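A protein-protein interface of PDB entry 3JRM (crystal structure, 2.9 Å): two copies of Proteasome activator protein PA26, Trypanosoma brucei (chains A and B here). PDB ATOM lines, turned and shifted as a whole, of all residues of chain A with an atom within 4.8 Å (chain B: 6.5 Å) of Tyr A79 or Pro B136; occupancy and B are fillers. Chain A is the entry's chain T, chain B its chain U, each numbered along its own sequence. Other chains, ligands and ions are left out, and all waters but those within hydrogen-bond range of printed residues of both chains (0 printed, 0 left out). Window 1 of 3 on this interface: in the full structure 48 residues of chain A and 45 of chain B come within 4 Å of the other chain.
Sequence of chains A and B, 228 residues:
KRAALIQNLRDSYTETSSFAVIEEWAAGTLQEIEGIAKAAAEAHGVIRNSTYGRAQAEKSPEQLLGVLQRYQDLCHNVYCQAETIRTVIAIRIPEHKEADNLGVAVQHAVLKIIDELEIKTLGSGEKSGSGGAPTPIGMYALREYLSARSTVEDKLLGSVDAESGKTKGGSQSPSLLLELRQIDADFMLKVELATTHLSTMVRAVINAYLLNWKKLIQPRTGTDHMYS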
ATOM      1  N   CYS A  75      26.716   5.919 -17.833  1.00  0.00           N
ATOM      2  CA  CYS A  75      26.688   6.118 -19.281  1.00  0.00           C
ATOM      3  C   CYS A  75      25.282   6.373 -19.807  1.00  0.00           C
ATOM      4  O   CYS A  75      25.103   7.238 -20.675  1.00  0.00           O
ATOM      5  CB  CYS A  75      27.315   4.921 -20.007  1.00  0.00           C
ATOM      6  SG  CYS A  75      29.103   4.716 -19.721  1.00  0.00           S
ATOM      7  N   HIS A  76      24.306   5.628 -19.267  1.00  0.00           N
ATOM      8  CA  HIS A  76      22.878   5.826 -19.561  1.00  0.00           C
ATOM      9  C   HIS A  76      22.428   7.258 -19.254  1.00  0.00           C
ATOM     10  O   HIS A  76      21.794   7.915 -20.085  1.00  0.00           O
ATOM     11  CB  HIS A  76      22.034   4.810 -18.770  1.00  0.00           C
ATOM     12  CG  HIS A  76      20.547   4.995 -18.883  1.00  0.00           C
ATOM     13  ND1 HIS A  76      19.676   4.517 -17.936  1.00  0.00           N
ATOM     14  CD2 HIS A  76      19.781   5.586 -19.827  1.00  0.00           C
ATOM     15  CE1 HIS A  76      18.439   4.796 -18.289  1.00  0.00           C
ATOM     16  NE2 HIS A  76      18.477   5.450 -19.434  1.00  0.00           N
ATOM     17  N   ASN A  77      22.758   7.746 -18.075  1.00  0.00           N
ATOM     18  CA  ASN A  77      22.353   9.090 -17.723  1.00  0.00           C
ATOM     19  C   ASN A  77      23.012  10.147 -18.584  1.00  0.00           C
ATOM     20  O   ASN A  77      22.363  11.066 -19.064  1.00  0.00           O
ATOM     21  CB  ASN A  77      22.619   9.357 -16.255  1.00  0.00           C
ATOM     22  CG  ASN A  77      21.864   8.420 -15.369  1.00  0.00           C
ATOM     23  OD1 ASN A  77      20.750   7.999 -15.690  1.00  0.00           O
ATOM     24  ND2 ASN A  77      22.468   8.062 -14.259  1.00  0.00           N
ATOM     25  N   VAL A  78      24.309  10.003 -18.791  1.00  0.00           N
ATOM     26  CA  VAL A  78      25.081  10.965 -19.589  1.00  0.00           C
ATOM     27  C   VAL A  78      24.536  11.027 -21.011  1.00  0.00           C
ATOM     28  O   VAL A  78      24.439  12.089 -21.579  1.00  0.00           O
ATOM     29  CB  VAL A  78      26.595  10.623 -19.573  1.00  0.00           C
ATOM     30  CG1 VAL A  78      27.341  11.380 -20.607  1.00  0.00           C
ATOM     31  CG2 VAL A  78      27.168  10.906 -18.200  1.00  0.00           C
ATOM     32  N   TYR A  79      24.153   9.889 -21.569  1.00  0.00           N
ATOM     33  CA  TYR A  79      23.536   9.873 -22.892  1.00  0.00           C
ATOM     34  C   TYR A  79      22.196  10.632 -22.932  1.00  0.00           C
ATOM     35  O   TYR A  79      21.946  11.396 -23.859  1.00  0.00           O
ATOM     36  CB  TYR A  79      23.327   8.442 -23.354  1.00  0.00           C
ATOM     37  CG  TYR A  79      22.838   8.266 -24.786  1.00  0.00           C
ATOM     38  CD1 TYR A  79      23.724   7.934 -25.814  1.00  0.00           C
ATOM     39  CD2 TYR A  79      21.492   8.357 -25.102  1.00  0.00           C
ATOM     40  CE1 TYR A  79      23.287   7.717 -27.122  1.00  0.00           C
ATOM     41  CE2 TYR A  79      21.046   8.148 -26.405  1.00  0.00           C
ATOM     42  CZ  TYR A  79      21.950   7.833 -27.407  1.00  0.00           C
ATOM     43  OH  TYR A  79      21.492   7.637 -28.676  1.00  0.00           O
ATOM     44  N   CYS A  80      21.336  10.414 -21.945  1.00  0.00           N
ATOM     45  CA  CYS A  80      20.042  11.071 -21.932  1.00  0.00           C
ATOM     46  C   CYS A  80      20.233  12.582 -21.737  1.00  0.00           C
ATOM     47  O   CYS A  80      19.557  13.397 -22.366  1.00  0.00           O
ATOM     48  CB  CYS A  80      19.129  10.430 -20.881  1.00  0.00           C
ATOM     49  SG  CYS A  80      18.487   8.787 -21.479  1.00  0.00           S
ATOM     50  N   GLN A  81      21.209  12.930 -20.910  1.00  0.00           N
ATOM     51  CA  GLN A  81      21.536  14.309 -20.626  1.00  0.00           C
ATOM     52  C   GLN A  81      22.173  15.013 -21.838  1.00  0.00           C
ATOM     53  O   GLN A  81      21.868  16.154 -22.142  1.00  0.00           O
ATOM     54  CB  GLN A  81      22.446  14.358 -19.392  1.00  0.00           C
ATOM     55  CG  GLN A  81      21.728  14.047 -18.078  1.00  0.00           C
ATOM     56  CD  GLN A  81      22.662  13.678 -16.936  1.00  0.00           C
ATOM     57  OE1 GLN A  81      23.730  13.101 -17.126  1.00  0.00           O
ATOM     58  NE2 GLN A  81      22.236  13.983 -15.736  1.00  0.00           N
ATOM     59  N   ALA A  82      23.067  14.315 -22.527  1.00  0.00           N
ATOM     60  CA  ALA A  82      23.662  14.794 -23.778  1.00  0.00           C
ATOM     61  C   ALA A  82      22.604  15.147 -24.795  1.00  0.00           C
ATOM     62  O   ALA A  82      22.691  16.180 -25.451  1.00  0.00           O
ATOM     63  CB  ALA A  82      24.581  13.749 -24.350  1.00  0.00           C
ATOM     64  N   GLU A  83      21.599  14.288 -24.907  1.00  0.00           N
ATOM     65  CA  GLU A  83      20.520  14.492 -25.861  1.00  0.00           C
ATOM     66  C   GLU A  83      19.655  15.720 -25.533  1.00  0.00           C
ATOM     67  O   GLU A  83      19.043  16.305 -26.437  1.00  0.00           O
ATOM     68  CB  GLU A  83      19.645  13.240 -25.970  1.00  0.00           C
ATOM     69  CG  GLU A  83      20.295  12.073 -26.719  1.00  0.00           C
ATOM     70  CD  GLU A  83      20.350  12.248 -28.232  1.00  0.00           C
ATOM     71  OE1 GLU A  83      19.473  12.842 -28.844  1.00  0.00           O
ATOM     72  OE2 GLU A  83      21.271  11.758 -28.855  1.00  0.00           O
ATOM     73  N   GLU A 118      28.585  10.735 -27.393  1.00  0.00           N
ATOM     74  CA  GLU A 118      27.570   9.679 -27.406  1.00  0.00           C
ATOM     75  C   GLU A 118      27.929   8.468 -28.271  1.00  0.00           C
ATOM     76  O   GLU A 118      27.819   7.335 -27.818  1.00  0.00           O
ATOM     77  CB  GLU A 118      26.256  10.223 -27.927  1.00  0.00           C
ATOM     78  CG  GLU A 118      25.594  11.226 -27.035  1.00  0.00           C
ATOM     79  CD  GLU A 118      24.271  11.638 -27.588  1.00  0.00           C
ATOM     80  OE1 GLU A 118      23.709  10.858 -28.395  1.00  0.00           O
ATOM     81  OE2 GLU A 118      23.810  12.739 -27.243  1.00  0.00           O
ATOM     82  N   LEU A 122      30.886   7.025 -25.404  1.00  0.00           N
ATOM     83  CA  LEU A 122      29.921   6.137 -24.749  1.00  0.00           C
ATOM     84  C   LEU A 122      29.681   4.826 -25.520  1.00  0.00           C
ATOM     85  O   LEU A 122      29.063   3.900 -24.988  1.00  0.00           O
ATOM     86  CB  LEU A 122      28.579   6.847 -24.480  1.00  0.00           C
ATOM     87  CG  LEU A 122      28.598   7.993 -23.463  1.00  0.00           C
ATOM     88  CD1 LEU A 122      27.251   8.666 -23.422  1.00  0.00           C
ATOM     89  CD2 LEU A 122      29.045   7.549 -22.067  1.00  0.00           C
ATOM     90  N   SER A 124      27.588   4.045 -27.776  1.00  0.00           N
ATOM     91  CA  SER A 124      26.152   3.832 -27.683  1.00  0.00           C
ATOM     92  C   SER A 124      25.552   3.112 -28.869  1.00  0.00           C
ATOM     93  O   SER A 124      24.476   2.550 -28.767  1.00  0.00           O
ATOM     94  CB  SER A 124      25.440   5.175 -27.508  1.00  0.00           C
ATOM     95  OG  SER A 124      25.587   6.010 -28.657  1.00  0.00           O
ATOM     96  N   GLY A 125      26.235   3.132 -29.997  1.00  0.00           N
ATOM     97  CA  GLY A 125      25.687   2.579 -31.219  1.00  0.00           C
ATOM     98  C   GLY A 125      25.692   1.072 -31.286  1.00  0.00           C
ATOM     99  O   GLY A 125      26.476   0.398 -30.639  1.00  0.00           O
ATOM    100  N   GLU A 126      24.810   0.562 -32.121  1.00  0.00           N
ATOM    101  CA  GLU A 126      24.630  -0.863 -32.352  1.00  0.00           C
ATOM    102  C   GLU A 126      25.847  -1.449 -33.068  1.00  0.00           C
ATOM    103  O   GLU A 126      26.237  -2.561 -32.812  1.00  0.00           O
ATOM    104  CB  GLU A 126      23.370  -1.043 -33.203  1.00  0.00           C
ATOM    105  CG  GLU A 126      22.736  -2.424 -33.268  1.00  0.00           C
ATOM    106  CD  GLU A 126      21.600  -2.448 -34.294  1.00  0.00           C
ATOM    107  OE1 GLU A 126      21.634  -3.282 -35.226  1.00  0.00           O
ATOM    108  OE2 GLU A 126      20.683  -1.598 -34.194  1.00  0.00           O
ATOM    109  N   TYR A 140      27.450  -1.132 -23.398  1.00  0.00           N
ATOM    110  CA  TYR A 140      26.969  -2.491 -23.246  1.00  0.00           C
ATOM    111  C   TYR A 140      28.109  -3.372 -22.728  1.00  0.00           C
ATOM    112  O   TYR A 140      28.410  -4.441 -23.295  1.00  0.00           O
ATOM    113  CB  TYR A 140      26.365  -2.967 -24.574  1.00  0.00           C
ATOM    114  CG  TYR A 140      25.504  -1.880 -25.191  1.00  0.00           C
ATOM    115  CD1 TYR A 140      25.788  -1.355 -26.443  1.00  0.00           C
ATOM    116  CD2 TYR A 140      24.449  -1.321 -24.477  1.00  0.00           C
ATOM    117  CE1 TYR A 140      25.023  -0.319 -26.984  1.00  0.00           C
ATOM    118  CE2 TYR A 140      23.681  -0.283 -25.007  1.00  0.00           C
ATOM    119  CZ  TYR A 140      23.982   0.214 -26.263  1.00  0.00           C
ATOM    120  OH  TYR A 140      23.225   1.228 -26.797  1.00  0.00           O
ATOM    121  N   THR B 121      19.097   6.834 -38.124  1.00  0.00           N
ATOM    122  CA  THR B 121      18.398   6.837 -36.833  1.00  0.00           C
ATOM    123  C   THR B 121      17.420   5.673 -36.750  1.00  0.00           C
ATOM    124  O   THR B 121      17.462   4.892 -35.808  1.00  0.00           O
ATOM    125  CB  THR B 121      17.656   8.185 -36.584  1.00  0.00           C
ATOM    126  OG1 THR B 121      18.588   9.253 -36.718  1.00  0.00           O
ATOM    127  CG2 THR B 121      17.031   8.272 -35.201  1.00  0.00           C
ATOM    128  N   ALA B 133      26.255   1.795 -37.490  1.00  0.00           N
ATOM    129  CA  ALA B 133      24.872   2.022 -37.122  1.00  0.00           C
ATOM    130  C   ALA B 133      24.884   2.774 -35.795  1.00  0.00           C
ATOM    131  O   ALA B 133      25.013   2.165 -34.740  1.00  0.00           O
ATOM    132  CB  ALA B 133      24.140   0.693 -37.004  1.00  0.00           C
ATOM    133  N   PRO B 134      24.792   4.110 -35.844  1.00  0.00           N
ATOM    134  CA  PRO B 134      24.958   4.920 -34.631  1.00  0.00           C
ATOM    135  C   PRO B 134      23.748   4.913 -33.691  1.00  0.00           C
ATOM    136  O   PRO B 134      23.859   5.324 -32.503  1.00  0.00           O
ATOM    137  CB  PRO B 134      25.178   6.323 -35.171  1.00  0.00           C
ATOM    138  CG  PRO B 134      24.506   6.321 -36.501  1.00  0.00           C
ATOM    139  CD  PRO B 134      24.573   4.940 -37.040  1.00  0.00           C
ATOM    140  N   THR B 135      22.601   4.457 -34.192  1.00  0.00           N
ATOM    141  CA  THR B 135      21.442   4.290 -33.331  1.00  0.00           C
ATOM    142  C   THR B 135      21.615   3.073 -32.423  1.00  0.00           C
ATOM    143  O   THR B 135      22.142   2.058 -32.859  1.00  0.00           O
ATOM    144  CB  THR B 135      20.155   4.128 -34.134  1.00  0.00           C
ATOM    145  OG1 THR B 135      19.063   4.108 -33.206  1.00  0.00           O
ATOM    146  CG2 THR B 135      20.161   2.839 -34.984  1.00  0.00           C
ATOM    147  N   PRO B 136      21.171   3.160 -31.163  1.00  0.00           N
ATOM    148  CA  PRO B 136      21.340   2.012 -30.276  1.00  0.00           C
ATOM    149  C   PRO B 136      20.591   0.752 -30.706  1.00  0.00           C
ATOM    150  O   PRO B 136      21.071  -0.353 -30.437  1.00  0.00           O
ATOM    151  CB  PRO B 136      20.825   2.530 -28.933  1.00  0.00           C
ATOM    152  CG  PRO B 136      20.938   4.022 -29.022  1.00  0.00           C
ATOM    153  CD  PRO B 136      20.625   4.325 -30.447  1.00  0.00           C
ATOM    154  N   ILE B 137      19.436   0.929 -31.362  1.00  0.00           N
ATOM    155  CA  ILE B 137      18.592  -0.180 -31.863  1.00  0.00           C
ATOM    156  C   ILE B 137      17.791   0.247 -33.100  1.00  0.00           C
ATOM    157  O   ILE B 137      17.300   1.368 -33.164  1.00  0.00           O
ATOM    158  CB  ILE B 137      17.648  -0.742 -30.746  1.00  0.00           C
ATOM    159  CG1 ILE B 137      17.152  -2.117 -31.127  1.00  0.00           C
ATOM    160  CG2 ILE B 137      16.440   0.162 -30.449  1.00  0.00           C
ATOM    161  CD1 ILE B 137      16.424  -2.780 -30.040  1.00  0.00           C
ATOM    162  N   GLY B 138      17.675  -0.650 -34.075  1.00  0.00           N
ATOM    163  CA  GLY B 138      17.029  -0.352 -35.346  1.00  0.00           C
ATOM    164  C   GLY B 138      15.548  -0.681 -35.436  1.00  0.00           C
ATOM    165  O   GLY B 138      14.936  -1.111 -34.463  1.00  0.00           O
ATOM    166  N   GLU B 144      16.167  -8.662 -33.789  1.00  0.00           N
ATOM    167  CA  GLU B 144      17.497  -8.660 -33.168  1.00  0.00           C
ATOM    168  C   GLU B 144      17.456  -9.328 -31.815  1.00  0.00           C
ATOM    169  O   GLU B 144      18.314 -10.134 -31.502  1.00  0.00           O
ATOM    170  CB  GLU B 144      18.054  -7.235 -32.990  1.00  0.00           C
ATOM    171  CG  GLU B 144      18.620  -6.523 -34.248  1.00  0.00           C
ATOM    172  CD  GLU B 144      19.113  -5.087 -33.909  1.00  0.00           C
ATOM    173  OE1 GLU B 144      18.567  -4.085 -34.466  1.00  0.00           O
ATOM    174  OE2 GLU B 144      20.043  -4.983 -33.056  1.00  0.00           O
ATOM    175  N   LEU B 189      17.061  -1.138 -22.307  1.00  0.00           N
ATOM    176  CA  LEU B 189      17.940   0.057 -22.257  1.00  0.00           C
ATOM    177  C   LEU B 189      18.064   0.667 -23.655  1.00  0.00           C
ATOM    178  O   LEU B 189      17.956   1.870 -23.825  1.00  0.00           O
ATOM    179  CB  LEU B 189      19.346  -0.287 -21.737  1.00  0.00           C
ATOM    180  CG  LEU B 189      20.380   0.853 -21.781  1.00  0.00           C
ATOM    181  CD1 LEU B 189      19.933   1.979 -20.915  1.00  0.00           C
ATOM    182  CD2 LEU B 189      21.758   0.382 -21.366  1.00  0.00           C
ATOM    183  N   LYS B 190      18.286  -0.186 -24.648  1.00  0.00           N
ATOM    184  CA  LYS B 190      18.476   0.273 -25.997  1.00  0.00           C
ATOM    185  C   LYS B 190      17.257   0.998 -26.513  1.00  0.00           C
ATOM    186  O   LYS B 190      17.391   1.948 -27.267  1.00  0.00           O
ATOM    187  CB  LYS B 190      18.873  -0.879 -26.929  1.00  0.00           C
ATOM    188  CG  LYS B 190      20.330  -1.336 -26.743  1.00  0.00           C
ATOM    189  CD  LYS B 190      20.752  -2.467 -27.689  1.00  0.00           C
ATOM    190  CE  LYS B 190      22.268  -2.736 -27.634  1.00  0.00           C
ATOM    191  NZ  LYS B 190      22.772  -3.514 -28.806  1.00  0.00           N
ATOM    192  N   VAL B 191      16.071   0.589 -26.091  1.00  0.00           N
ATOM    193  CA  VAL B 191      14.851   1.309 -26.474  1.00  0.00           C
ATOM    194  C   VAL B 191      14.721   2.669 -25.750  1.00  0.00           C
ATOM    195  O   VAL B 191      14.238   3.611 -26.367  1.00  0.00           O
ATOM    196  CB  VAL B 191      13.571   0.444 -26.276  1.00  0.00           C
ATOM    197  CG1 VAL B 191      12.316   1.260 -26.597  1.00  0.00           C
ATOM    198  CG2 VAL B 191      13.640  -0.788 -27.155  1.00  0.00           C
ATOM    199  N   GLU B 192      15.135   2.779 -24.480  1.00  0.00           N
ATOM    200  CA  GLU B 192      15.128   4.070 -23.804  1.00  0.00           C
ATOM    201  C   GLU B 192      16.028   5.018 -24.548  1.00  0.00           C
ATOM    202  O   GLU B 192      15.626   6.139 -24.853  1.00  0.00           O
ATOM    203  CB  GLU B 192      15.655   4.011 -22.364  1.00  0.00           C
ATOM    204  CG  GLU B 192      14.869   3.172 -21.386  1.00  0.00           C
ATOM    205  CD  GLU B 192      15.494   3.220 -20.019  1.00  0.00           C
ATOM    206  OE1 GLU B 192      15.743   2.114 -19.445  1.00  0.00           O
ATOM    207  OE2 GLU B 192      15.750   4.366 -19.568  1.00  0.00           O
ATOM    208  N   LEU B 193      17.259   4.571 -24.814  1.00  0.00           N
ATOM    209  CA  LEU B 193      18.274   5.383 -25.504  1.00  0.00           C
ATOM    210  C   LEU B 193      17.828   5.725 -26.935  1.00  0.00           C
ATOM    211  O   LEU B 193      17.874   6.872 -27.359  1.00  0.00           O
ATOM    212  CB  LEU B 193      19.621   4.657 -25.526  1.00  0.00           C
ATOM    213  CG  LEU B 193      20.249   4.255 -24.177  1.00  0.00           C
ATOM    214  CD1 LEU B 193      21.594   3.606 -24.406  1.00  0.00           C
ATOM    215  CD2 LEU B 193      20.392   5.415 -23.211  1.00  0.00           C
ATOM    216  N   ALA B 194      17.359   4.729 -27.669  1.00  0.00           N
ATOM    217  CA  ALA B 194      16.951   4.959 -29.037  1.00  0.00           C
ATOM    218  C   ALA B 194      15.803   5.966 -29.111  1.00  0.00           C
ATOM    219  O   ALA B 194      15.776   6.789 -30.009  1.00  0.00           O
ATOM    220  CB  ALA B 194      16.580   3.661 -29.710  1.00  0.00           C
ATOM    221  N   THR B 195      14.864   5.921 -28.165  1.00  0.00           N
ATOM    222  CA  THR B 195      13.732   6.830 -28.195  1.00  0.00           C
ATOM    223  C   THR B 195      14.182   8.269 -27.914  1.00  0.00           C
ATOM    224  O   THR B 195      13.726   9.160 -28.616  1.00  0.00           O
ATOM    225  CB  THR B 195      12.563   6.377 -27.258  1.00  0.00           C
ATOM    226  OG1 THR B 195      13.075   6.044 -25.966  1.00  0.00           O
ATOM    227  CG2 THR B 195      11.824   5.189 -27.842  1.00  0.00           C
ATOM    228  N   THR B 196      15.072   8.503 -26.939  1.00  0.00           N
ATOM    229  CA  THR B 196      15.603   9.869 -26.706  1.00  0.00           C
ATOM    230  C   THR B 196      16.251  10.395 -27.970  1.00  0.00           C
ATOM    231  O   THR B 196      15.985  11.521 -28.392  1.00  0.00           O
ATOM    232  CB  THR B 196      16.676   9.967 -25.605  1.00  0.00           C
ATOM    233  OG1 THR B 196      16.437   8.996 -24.596  1.00  0.00           O
ATOM    234  CG2 THR B 196      16.673  11.333 -24.944  1.00  0.00           C
ATOM    235  N   HIS B 197      17.108   9.569 -28.558  1.00  0.00           N
ATOM    236  CA  HIS B 197      17.819   9.896 -29.786  1.00  0.00           C
ATOM    237  C   HIS B 197      16.856  10.235 -30.898  1.00  0.00           C
ATOM    238  O   HIS B 197      17.036  11.260 -31.558  1.00  0.00           O
ATOM    239  CB  HIS B 197      18.688   8.730 -30.207  1.00  0.00           C
ATOM    240  CG  HIS B 197      19.714   9.072 -31.241  1.00  0.00           C
ATOM    241  ND1 HIS B 197      20.839   9.812 -30.953  1.00  0.00           N
ATOM    242  CD2 HIS B 197      19.814   8.726 -32.547  1.00  0.00           C
ATOM    243  CE1 HIS B 197      21.579   9.922 -32.038  1.00  0.00           C
ATOM    244  NE2 HIS B 197      20.971   9.282 -33.023  1.00  0.00           N
ATOM    245  N   LEU B 198      15.820   9.406 -31.085  1.00  0.00           N
ATOM    246  CA  LEU B 198      14.790   9.651 -32.122  1.00  0.00           C
ATOM    247  C   LEU B 198      14.008  10.963 -31.888  1.00  0.00           C
ATOM    248  O   LEU B 198      13.601  11.646 -32.824  1.00  0.00           O
ATOM    249  CB  LEU B 198      13.820   8.472 -32.205  1.00  0.00           C
ATOM    250  CG  LEU B 198      12.697   8.580 -33.244  1.00  0.00           C
ATOM    251  CD1 LEU B 198      13.266   8.697 -34.615  1.00  0.00           C
ATOM    252  CD2 LEU B 198      11.755   7.408 -33.161  1.00  0.00           C
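No position is printed for both chains.
Among the printed residues, pairs that only touch across the chains: Glu A126 with Ile B137, His A76 with Leu B193, Tyr A140 with Pro B136, Ser A124 with Pro B136, Gly A125 with Pro B134, Tyr A79 with Leu B193, Gly A125 with Ala B133, Glu A126 with Pro B136, Tyr A79 with Pro B136, Tyr A140 with Lys B190, Glu A83 with Thr B196, His A76 with Leu B189, Tyr A140 with Leu B193, Gly A125 with Thr B135 and Glu A118 with His B197.
Printed residues of chain A that touch a printed residue of chain B: His A76, Tyr A79, Cys A80, Glu A83, Glu A118, Ser A124, Gly A125, Glu A126 and Tyr A140. Hydrophobic or aromatic side chains of chain B within 4 Å of the printed part of chain A: Pro B136, Leu B189, Leu B193 and His B197. Among the printed residues, 23 pairs touch across the chains. Among the printed residues, no Asp or Glu carboxylate lies within 4 Å of a Lys or Arg side-chain nitrogen of the other chain.
SG of Cys A80 lies within hydrogen-bond range of OG1 of Thr B196 (3.7 Å). N of Glu A126 is in hydrogen-bond range of O of Ala B133. A ring nitrogen (NE2) of His A76 lies within hydrogen-bond range of the side-chain carboxylate (OE2) of Glu B192 (2.9 Å). O of Thr B135 sits at hydrogen-bond distance from N of Glu A126, at 3.1 Å. OH of Tyr A79 lies within hydrogen-bond range of ND1 of His B197, at 3.2 Å. OE1 of Glu A126 sits close to OE2 of Glu B144, at 3.2 Å. The side-chain carboxylate (OE2) of Glu A83 is in hydrogen-bond range of a ring nitrogen (ND1) of His B197 (2.9 Å). The backbone NH of Gly B138 is in hydrogen-bond range of the side-chain carboxylate of Glu A126 (3.2 Å).
The side-chain carboxylate (OE1) of Glu A118 lies close to the side-chain carboxylate (OE2) of Glu A83 (2.6 Å). O of Ser A124 is in hydrogen-bond range of OH of Tyr A140 (2.7 Å). O of Glu B192 is in hydrogen-bond range of OG1 of Thr B196, 3.0 Å away. O of Glu B192 lies within hydrogen-bond range of OG1 of Thr B195, 2.8 Å away. OG1 of Thr B135 is in hydrogen-bond range of O of Thr B121 (3.2 Å). The side-chain sulfur (SG) of Cys A80 lies within hydrogen-bond range of the backbone carbonyl oxygen (O) of His A76, 3.7 Å away.
Pro B136 touches four residues of chain A. Printed residues of chain A within 4 Å of Lys B190: Tyr A140 (3.7 Å). Ala B194 touches none of the printed residues of chain A. Of the printed residues of chain A, His B197 touches Tyr A79, Glu A83 and Glu A118. Leu B198 touches none of the printed residues of chain A. The nearest residue of chain B that does not touch Tyr A79 is Thr B196 (4.8 Å).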
